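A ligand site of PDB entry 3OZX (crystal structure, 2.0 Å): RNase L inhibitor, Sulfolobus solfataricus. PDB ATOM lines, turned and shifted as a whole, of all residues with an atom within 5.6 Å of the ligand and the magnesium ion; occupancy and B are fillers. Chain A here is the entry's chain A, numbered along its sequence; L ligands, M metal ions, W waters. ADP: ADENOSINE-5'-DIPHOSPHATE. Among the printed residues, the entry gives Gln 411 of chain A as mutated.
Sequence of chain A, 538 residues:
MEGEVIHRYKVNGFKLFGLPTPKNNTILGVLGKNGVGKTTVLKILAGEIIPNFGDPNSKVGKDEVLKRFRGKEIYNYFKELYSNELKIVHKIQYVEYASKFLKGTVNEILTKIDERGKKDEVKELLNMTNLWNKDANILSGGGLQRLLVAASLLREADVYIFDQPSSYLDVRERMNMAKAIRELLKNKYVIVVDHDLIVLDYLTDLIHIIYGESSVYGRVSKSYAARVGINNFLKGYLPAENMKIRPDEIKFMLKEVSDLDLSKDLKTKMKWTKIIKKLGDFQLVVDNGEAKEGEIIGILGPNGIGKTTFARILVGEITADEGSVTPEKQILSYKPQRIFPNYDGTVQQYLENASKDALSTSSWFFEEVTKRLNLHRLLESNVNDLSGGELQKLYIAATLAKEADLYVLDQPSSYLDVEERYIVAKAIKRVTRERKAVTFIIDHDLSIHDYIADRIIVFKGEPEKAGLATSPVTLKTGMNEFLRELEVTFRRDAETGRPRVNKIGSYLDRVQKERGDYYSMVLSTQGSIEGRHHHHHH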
ATOM      1  N   LEU A 279     -14.990   8.895 -17.540  1.00  0.00           N
ATOM      2  CA  LEU A 279     -15.331   8.539 -18.936  1.00  0.00           C
ATOM      3  C   LEU A 279     -14.053   8.483 -19.735  1.00  0.00           C
ATOM      4  O   LEU A 279     -13.500   9.535 -20.115  1.00  0.00           O
ATOM      5  CB  LEU A 279     -16.324   9.532 -19.593  1.00  0.00           C
ATOM      6  CG  LEU A 279     -17.652   9.837 -18.920  1.00  0.00           C
ATOM      7  CD1 LEU A 279     -18.238  11.162 -19.536  1.00  0.00           C
ATOM      8  CD2 LEU A 279     -18.634   8.639 -19.079  1.00  0.00           C
ATOM      9  N   GLY A 280     -13.562   7.272 -19.960  1.00  0.00           N
ATOM     10  CA  GLY A 280     -12.360   7.054 -20.750  1.00  0.00           C
ATOM     11  C   GLY A 280     -11.214   7.776 -20.081  1.00  0.00           C
ATOM     12  O   GLY A 280     -10.925   7.532 -18.916  1.00  0.00           O
ATOM     13  N   ASP A 281     -10.593   8.703 -20.795  1.00  0.00           N
ATOM     14  CA  ASP A 281      -9.501   9.480 -20.222  1.00  0.00           C
ATOM     15  C   ASP A 281     -10.000  10.462 -19.141  1.00  0.00           C
ATOM     16  O   ASP A 281      -9.368  10.635 -18.106  1.00  0.00           O
ATOM     17  CB  ASP A 281      -8.576  10.117 -21.307  1.00  0.00           C
ATOM     18  CG  ASP A 281      -9.347  10.806 -22.458  1.00  0.00           C
ATOM     19  OD1 ASP A 281     -10.576  10.586 -22.625  1.00  0.00           O
ATOM     20  OD2 ASP A 281      -8.707  11.596 -23.203  1.00  0.00           O
ATOM     21  N   PHE A 282     -11.195  11.001 -19.339  1.00  0.00           N
ATOM     22  CA  PHE A 282     -11.685  12.106 -18.566  1.00  0.00           C
ATOM     23  C   PHE A 282     -12.212  11.705 -17.197  1.00  0.00           C
ATOM     24  O   PHE A 282     -13.014  10.797 -17.104  1.00  0.00           O
ATOM     25  CB  PHE A 282     -12.820  12.799 -19.364  1.00  0.00           C
ATOM     26  CG  PHE A 282     -13.517  13.904 -18.584  1.00  0.00           C
ATOM     27  CD1 PHE A 282     -12.889  15.140 -18.380  1.00  0.00           C
ATOM     28  CD2 PHE A 282     -14.810  13.731 -18.110  1.00  0.00           C
ATOM     29  CE1 PHE A 282     -13.507  16.158 -17.713  1.00  0.00           C
ATOM     30  CE2 PHE A 282     -15.435  14.760 -17.432  1.00  0.00           C
ATOM     31  CZ  PHE A 282     -14.785  15.977 -17.257  1.00  0.00           C
ATOM     32  N   PRO A 302     -15.325  26.207 -18.966  1.00  0.00           N
ATOM     33  CA  PRO A 302     -14.924  25.972 -20.387  1.00  0.00           C
ATOM     34  C   PRO A 302     -15.501  24.676 -20.995  1.00  0.00           C
ATOM     35  O   PRO A 302     -15.954  23.792 -20.267  1.00  0.00           O
ATOM     36  CB  PRO A 302     -13.373  25.942 -20.331  1.00  0.00           C
ATOM     37  CG  PRO A 302     -13.027  25.546 -18.891  1.00  0.00           C
ATOM     38  CD  PRO A 302     -14.246  25.935 -17.982  1.00  0.00           C
ATOM     39  N   ASN A 303     -15.531  24.515 -22.335  1.00  0.00           N
ATOM     40  CA  ASN A 303     -16.092  23.228 -22.772  1.00  0.00           C
ATOM     41  C   ASN A 303     -15.142  22.061 -22.554  1.00  0.00           C
ATOM     42  O   ASN A 303     -13.943  22.245 -22.568  1.00  0.00           O
ATOM     43  CB  ASN A 303     -16.587  23.306 -24.216  1.00  0.00           C
ATOM     44  CG  ASN A 303     -17.905  23.993 -24.294  1.00  0.00           C
ATOM     45  OD1 ASN A 303     -18.677  24.032 -23.310  1.00  0.00           O
ATOM     46  ND2 ASN A 303     -18.189  24.563 -25.438  1.00  0.00           N
ATOM     47  N   GLY A 304     -15.684  20.852 -22.387  1.00  0.00           N
ATOM     48  CA  GLY A 304     -14.885  19.634 -22.303  1.00  0.00           C
ATOM     49  C   GLY A 304     -14.538  19.299 -20.870  1.00  0.00           C
ATOM     50  O   GLY A 304     -13.704  18.422 -20.608  1.00  0.00           O
ATOM     51  N   ILE A 305     -15.270  19.929 -19.971  1.00  0.00           N
ATOM     52  CA  ILE A 305     -14.944  19.972 -18.572  1.00  0.00           C
ATOM     53  C   ILE A 305     -15.947  19.181 -17.701  1.00  0.00           C
ATOM     54  O   ILE A 305     -15.704  18.980 -16.540  1.00  0.00           O
ATOM     55  CB  ILE A 305     -14.891  21.482 -18.095  1.00  0.00           C
ATOM     56  CG1 ILE A 305     -13.777  21.666 -17.070  1.00  0.00           C
ATOM     57  CG2 ILE A 305     -16.233  21.908 -17.482  1.00  0.00           C
ATOM     58  CD1 ILE A 305     -12.349  21.227 -17.671  1.00  0.00           C
ATOM     59  N   GLY A 306     -17.076  18.743 -18.279  1.00  0.00           N
ATOM     60  CA  GLY A 306     -17.932  17.771 -17.590  1.00  0.00           C
ATOM     61  C   GLY A 306     -19.287  18.323 -17.201  1.00  0.00           C
ATOM     62  O   GLY A 306     -20.031  17.671 -16.470  1.00  0.00           O
ATOM     63  N   LYS A 307     -19.604  19.539 -17.646  1.00  0.00           N
ATOM     64  CA  LYS A 307     -20.910  20.147 -17.334  1.00  0.00           C
ATOM     65  C   LYS A 307     -22.107  19.308 -17.845  1.00  0.00           C
ATOM     66  O   LYS A 307     -23.049  19.017 -17.103  1.00  0.00           O
ATOM     67  CB  LYS A 307     -20.967  21.612 -17.863  1.00  0.00           C
ATOM     68  CG  LYS A 307     -19.718  22.446 -17.643  1.00  0.00           C
ATOM     69  CD  LYS A 307     -19.922  23.965 -18.234  1.00  0.00           C
ATOM     70  CE  LYS A 307     -20.107  23.933 -19.765  1.00  0.00           C
ATOM     71  NZ  LYS A 307     -18.825  23.592 -20.380  1.00  0.00           N
ATOM     72  N   THR A 308     -22.078  18.922 -19.115  1.00  0.00           N
ATOM     73  CA  THR A 308     -23.067  18.022 -19.699  1.00  0.00           C
ATOM     74  C   THR A 308     -23.092  16.635 -19.078  1.00  0.00           C
ATOM     75  O   THR A 308     -24.186  16.094 -18.814  1.00  0.00           O
ATOM     76  CB  THR A 308     -22.858  17.880 -21.199  1.00  0.00           C
ATOM     77  OG1 THR A 308     -23.119  19.146 -21.822  1.00  0.00           O
ATOM     78  CG2 THR A 308     -23.828  16.866 -21.819  1.00  0.00           C
ATOM     79  N   THR A 309     -21.911  16.100 -18.773  1.00  0.00           N
ATOM     80  CA  THR A 309     -21.836  14.851 -18.026  1.00  0.00           C
ATOM     81  C   THR A 309     -22.591  15.018 -16.721  1.00  0.00           C
ATOM     82  O   THR A 309     -23.331  14.146 -16.292  1.00  0.00           O
ATOM     83  CB  THR A 309     -20.377  14.476 -17.773  1.00  0.00           C
ATOM     84  OG1 THR A 309     -19.798  14.267 -19.071  1.00  0.00           O
ATOM     85  CG2 THR A 309     -20.224  13.197 -16.908  1.00  0.00           C
ATOM     86  N   PHE A 310     -22.413  16.167 -16.078  1.00  0.00           N
ATOM     87  CA  PHE A 310     -23.029  16.368 -14.763  1.00  0.00           C
ATOM     88  C   PHE A 310     -24.566  16.444 -14.967  1.00  0.00           C
ATOM     89  O   PHE A 310     -25.317  15.696 -14.385  1.00  0.00           O
ATOM     90  CB  PHE A 310     -22.508  17.632 -14.106  1.00  0.00           C
ATOM     91  CG  PHE A 310     -23.158  17.930 -12.775  1.00  0.00           C
ATOM     92  CD1 PHE A 310     -23.257  16.949 -11.798  1.00  0.00           C
ATOM     93  CD2 PHE A 310     -23.686  19.193 -12.511  1.00  0.00           C
ATOM     94  CE1 PHE A 310     -23.870  17.235 -10.569  1.00  0.00           C
ATOM     95  CE2 PHE A 310     -24.278  19.473 -11.305  1.00  0.00           C
ATOM     96  CZ  PHE A 310     -24.365  18.500 -10.327  1.00  0.00           C
ATOM     97  N   ARG A 312     -26.212  15.044 -17.274  1.00  0.00           N
ATOM     98  CA  ARG A 312     -26.677  13.729 -17.651  1.00  0.00           C
ATOM     99  C   ARG A 312     -26.806  12.868 -16.390  1.00  0.00           C
ATOM    100  O   ARG A 312     -27.709  12.070 -16.289  1.00  0.00           O
ATOM    101  CB  ARG A 312     -25.762  13.088 -18.720  1.00  0.00           C
ATOM    102  CG  ARG A 312     -25.981  13.587 -20.152  1.00  0.00           C
ATOM    103  CD  ARG A 312     -25.021  12.916 -21.140  1.00  0.00           C
ATOM    104  NE  ARG A 312     -25.307  13.386 -22.490  1.00  0.00           N
ATOM    105  CZ  ARG A 312     -24.464  13.356 -23.515  1.00  0.00           C
ATOM    106  NH1 ARG A 312     -23.236  12.873 -23.398  1.00  0.00           N
ATOM    107  NH2 ARG A 312     -24.872  13.821 -24.680  1.00  0.00           N
ATOM    108  N   ILE A 318     -26.875   9.076 -17.348  1.00  0.00           N
ATOM    109  CA  ILE A 318     -25.594   8.436 -17.066  1.00  0.00           C
ATOM    110  C   ILE A 318     -25.615   8.157 -15.552  1.00  0.00           C
ATOM    111  O   ILE A 318     -26.240   8.910 -14.795  1.00  0.00           O
ATOM    112  CB  ILE A 318     -24.397   9.331 -17.527  1.00  0.00           C
ATOM    113  CG1 ILE A 318     -24.145   9.127 -19.034  1.00  0.00           C
ATOM    114  CG2 ILE A 318     -23.140   8.982 -16.742  1.00  0.00           C
ATOM    115  CD1 ILE A 318     -23.002  10.045 -19.679  1.00  0.00           C
ATOM    116  N   GLN A 337     -28.142  19.774 -24.500  1.00  0.00           N
ATOM    117  CA  GLN A 337     -27.306  20.665 -25.269  1.00  0.00           C
ATOM    118  C   GLN A 337     -27.481  20.395 -26.743  1.00  0.00           C
ATOM    119  O   GLN A 337     -27.730  21.336 -27.488  1.00  0.00           O
ATOM    120  CB  GLN A 337     -25.848  20.562 -24.889  1.00  0.00           C
ATOM    121  CG  GLN A 337     -24.841  21.311 -25.815  1.00  0.00           C
ATOM    122  CD  GLN A 337     -23.416  21.138 -25.284  1.00  0.00           C
ATOM    123  OE1 GLN A 337     -22.439  21.303 -26.020  1.00  0.00           O
ATOM    124  NE2 GLN A 337     -23.308  20.853 -23.995  1.00  0.00           N
ATOM    125  N   ASP A 410     -29.510  22.771 -20.832  1.00  0.00           N
ATOM    126  CA  ASP A 410     -28.101  22.723 -21.189  1.00  0.00           C
ATOM    127  C   ASP A 410     -27.774  23.693 -22.351  1.00  0.00           C
ATOM    128  O   ASP A 410     -28.148  23.424 -23.478  1.00  0.00           O
ATOM    129  CB  ASP A 410     -27.687  21.281 -21.522  1.00  0.00           C
ATOM    130  CG  ASP A 410     -26.146  21.094 -21.534  1.00  0.00           C
ATOM    131  OD1 ASP A 410     -25.429  22.119 -21.494  1.00  0.00           O
ATOM    132  OD2 ASP A 410     -25.650  19.922 -21.590  1.00  0.00           O
ATOM    133  N   GLN A 411     -27.072  24.793 -22.073  1.00  0.00           N
ATOM    134  CA  GLN A 411     -26.708  25.768 -23.148  1.00  0.00           C
ATOM    135  C   GLN A 411     -27.908  26.307 -23.936  1.00  0.00           C
ATOM    136  O   GLN A 411     -27.873  26.358 -25.129  1.00  0.00           O
ATOM    137  CB  GLN A 411     -25.618  25.182 -24.116  1.00  0.00           C
ATOM    138  CG  GLN A 411     -24.371  24.698 -23.302  1.00  0.00           C
ATOM    139  CD  GLN A 411     -23.105  24.510 -24.058  1.00  0.00           C
ATOM    140  OE1 GLN A 411     -23.009  24.844 -25.247  1.00  0.00           O
ATOM    141  NE2 GLN A 411     -22.087  24.012 -23.371  1.00  0.00           N
ATOM    142  N   PRO A 463      -9.833  20.791 -20.095  1.00  0.00           N
ATOM    143  CA  PRO A 463     -10.735  20.161 -21.043  1.00  0.00           C
ATOM    144  C   PRO A 463     -10.239  18.815 -21.479  1.00  0.00           C
ATOM    145  O   PRO A 463      -9.069  18.651 -21.772  1.00  0.00           O
ATOM    146  CB  PRO A 463     -10.781  21.171 -22.194  1.00  0.00           C
ATOM    147  CG  PRO A 463     -10.745  22.511 -21.452  1.00  0.00           C
ATOM    148  CD  PRO A 463      -9.728  22.249 -20.319  1.00  0.00           C
ATOM    149  N   GLU A 464     -11.133  17.833 -21.451  1.00  0.00           N
ATOM    150  CA  GLU A 464     -10.901  16.483 -21.957  1.00  0.00           C
ATOM    151  C   GLU A 464     -10.181  15.537 -20.999  1.00  0.00           C
ATOM    152  O   GLU A 464     -10.163  14.328 -21.231  1.00  0.00           O
ATOM    153  CB  GLU A 464     -10.146  16.529 -23.304  1.00  0.00           C
ATOM    154  CG  GLU A 464     -10.310  15.280 -24.179  1.00  0.00           C
ATOM    155  CD  GLU A 464      -9.509  15.334 -25.490  1.00  0.00           C
ATOM    156  OE1 GLU A 464      -8.277  15.045 -25.476  1.00  0.00           O
ATOM    157  OE2 GLU A 464     -10.112  15.642 -26.543  1.00  0.00           O
ATOM    158  N   LYS A 465      -9.601  16.070 -19.918  1.00  0.00           N
ATOM    159  CA  LYS A 465      -8.727  15.228 -19.074  1.00  0.00           C
ATOM    160  C   LYS A 465      -9.292  15.153 -17.641  1.00  0.00           C
ATOM    161  O   LYS A 465      -9.459  14.073 -17.088  1.00  0.00           O
ATOM    162  CB  LYS A 465      -7.300  15.788 -19.038  1.00  0.00           C
ATOM    163  CG  LYS A 465      -6.583  15.939 -20.373  1.00  0.00           C
ATOM    164  CD  LYS A 465      -5.858  14.692 -20.723  1.00  0.00           C
ATOM    165  CE  LYS A 465      -5.172  14.828 -22.111  1.00  0.00           C
ATOM    166  NZ  LYS A 465      -5.786  13.857 -23.045  1.00  0.00           N
HETATM  167  PB  ADP L   1     -18.946  20.051 -21.420  1.00  0.00           P
HETATM  168  O1B ADP L   1     -20.483  19.982 -21.318  1.00  0.00           O
HETATM  169  O2B ADP L   1     -18.372  20.726 -20.248  1.00  0.00           O
HETATM  170  O3B ADP L   1     -18.413  20.492 -22.723  1.00  0.00           O
HETATM  171  PA  ADP L   1     -18.971  17.082 -21.367  1.00  0.00           P
HETATM  172  O1A ADP L   1     -19.504  16.544 -20.086  1.00  0.00           O
HETATM  173  O2A ADP L   1     -19.604  16.936 -22.785  1.00  0.00           O
HETATM  174  O3A ADP L   1     -18.287  18.575 -21.295  1.00  0.00           O
HETATM  175  O5' ADP L   1     -17.642  16.342 -21.703  1.00  0.00           O
HETATM  176  C5' ADP L   1     -16.651  15.975 -20.742  1.00  0.00           C
HETATM  177  C4' ADP L   1     -15.535  15.195 -21.454  1.00  0.00           C
HETATM  178  O4' ADP L   1     -15.932  13.807 -21.498  1.00  0.00           O
HETATM  179  C3' ADP L   1     -15.302  15.625 -22.883  1.00  0.00           C
HETATM  180  O3' ADP L   1     -13.877  15.564 -23.168  1.00  0.00           O
HETATM  181  C2' ADP L   1     -15.986  14.539 -23.722  1.00  0.00           C
HETATM  182  O2' ADP L   1     -15.296  14.280 -24.951  1.00  0.00           O
HETATM  183  C1' ADP L   1     -15.910  13.298 -22.851  1.00  0.00           C
HETATM  184  N9  ADP L   1     -17.119  12.452 -22.972  1.00  0.00           N
HETATM  185  C8  ADP L   1     -18.428  12.836 -22.926  1.00  0.00           C
HETATM  186  N7  ADP L   1     -19.215  11.752 -23.032  1.00  0.00           N
HETATM  187  C5  ADP L   1     -18.389  10.687 -23.104  1.00  0.00           C
HETATM  188  C6  ADP L   1     -18.580   9.303 -23.215  1.00  0.00           C
HETATM  189  N6  ADP L   1     -19.812   8.773 -23.288  1.00  0.00           N
HETATM  190  N1  ADP L   1     -17.511   8.496 -23.310  1.00  0.00           N
HETATM  191  C2  ADP L   1     -16.244   8.975 -23.233  1.00  0.00           C
HETATM  192  N3  ADP L   1     -16.008  10.307 -23.109  1.00  0.00           N
HETATM  193  C4  ADP L   1     -17.069  11.141 -23.056  1.00  0.00           C
HETATM  194 MG    MG M   1     -21.844  20.354 -22.791  1.00  0.00          MG
HETATM  195  O   HOH W   1     -20.818  14.688 -23.487  1.00  0.00           O
HETATM  196  O   HOH W   2     -21.116  18.938 -23.758  1.00  0.00           O
HETATM  197  O   HOH W   3     -20.598  21.571 -23.893  1.00  0.00           O
HETATM  198  O   HOH W   4     -13.327  10.726 -22.831  1.00  0.00           O
HETATM  199  O   HOH W   5     -21.339  12.786 -20.890  1.00  0.00           O
HETATM  200  O   HOH W   6     -12.613  17.141 -25.095  1.00  0.00           O
HETATM  201  O   HOH W   7     -22.511  21.794 -21.840  1.00  0.00           O
HETATM  202  O   HOH W   8     -15.303  17.499 -25.548  1.00  0.00           O
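Gln 411 touches the magnesium ion. Within 4 Å of the magnesium ion: Thr 308, Gln 337 and Gln 411.
O of Gly 304 lies within hydrogen-bond range of N of Glu 464, 2.8 Å away. OD2 of Asp 410 lies close to OG1 of Thr 308 (2.7 Å). The backbone carbonyl oxygen of Pro 302 is in hydrogen-bond range of the side-chain amino group of Lys 307, 2.9 Å away. The side-chain amide oxygen (OD1) of Asn 303 sits at hydrogen-bond distance from the side-chain amino group (NZ) of Lys 307 (3.0 Å). NE2 of Gln 411 is in hydrogen-bond range of OD1 of Asn 303 (3.4 Å). NZ of Lys 465 lies within salt-bridge range of OE1 of Glu 464, 3.7 Å away. NE2 of Gln 337 sits close to OD2 of Asp 410, 3.5 Å away. The side-chain amide nitrogen (NE2) of Gln 337 sits close to the side-chain amide nitrogen (NE2) of Gln 411 (3.4 Å).
Water W3 lies within hydrogen-bond range of O3B of the ligand (2.7 Å), OE1 of Gln 337 (2.8 Å), NE2 of Gln 411 (2.9 Å) and OD1 of Asn 303 (3.2 Å). Water W7 lies within hydrogen-bond range of NE2 of Gln 411 and OD1 of Asp 410. Water W1 lies within hydrogen-bond range of an oxygen (O2A) of the ligand (2.6 Å) and the guanidinium group (NH1) of Arg 312 (3.0 Å). Water W6 lies within hydrogen-bond range of an oxygen (O3') of the ligand (2.8 Å) and the side-chain carboxylate of Glu 464 (3.3 Å). Water W5 lies within hydrogen-bond range of OG1 of Thr 309 (2.8 Å), NH1 of Arg 312 (3.1 Å) and N7 of the ligand (3.2 Å).
The backbone NH (N) of Gly 304 is in hydrogen-bond range of an oxygen (O3B) of the ligand, at 2.8 Å. The backbone NH of Gly 306 is in hydrogen-bond range of an oxygen (O2B) of the ligand, at 3.1 Å. The side-chain hydroxyl of Thr 309 sits at hydrogen-bond distance from an oxygen (O1A) of the ligand (2.5 Å). The side-chain amino group of Lys 307 lies within salt-bridge range of an oxygen (O2B) of the ligand. O1B of the ligand sits close to N of Thr 308, 2.9 Å away. O2B of the ligand is in hydrogen-bond range of N of Ile 305 (3.2 Å). N of Lys 307 sits at hydrogen-bond distance from O2B of the ligand (3.1 Å). N of Thr 309 lies within hydrogen-bond range of O1A of the ligand, at 2.8 Å.
Merely in contact with the ligand: Glu 464 (3.3 Å), Phe 282 (3.6 Å), Asn 303 (3.6 Å), Leu 279 (3.6 Å) and Pro 302 (3.9 Å). Hydrophobic or aromatic side chains within 4 Å of the ligand: Leu 279, Phe 282 and Ile 305. The nearest printed residue that does not touch the ligand is Arg 312 (4.2 Å).
The magnesium ion is bound by water W7, water W2, the side-chain amide nitrogen of Gln 337, the side-chain hydroxyl of Thr 308, an oxygen (O1B) of the ligand and water W3. The magnesium ion has six donor atoms within binding distance.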
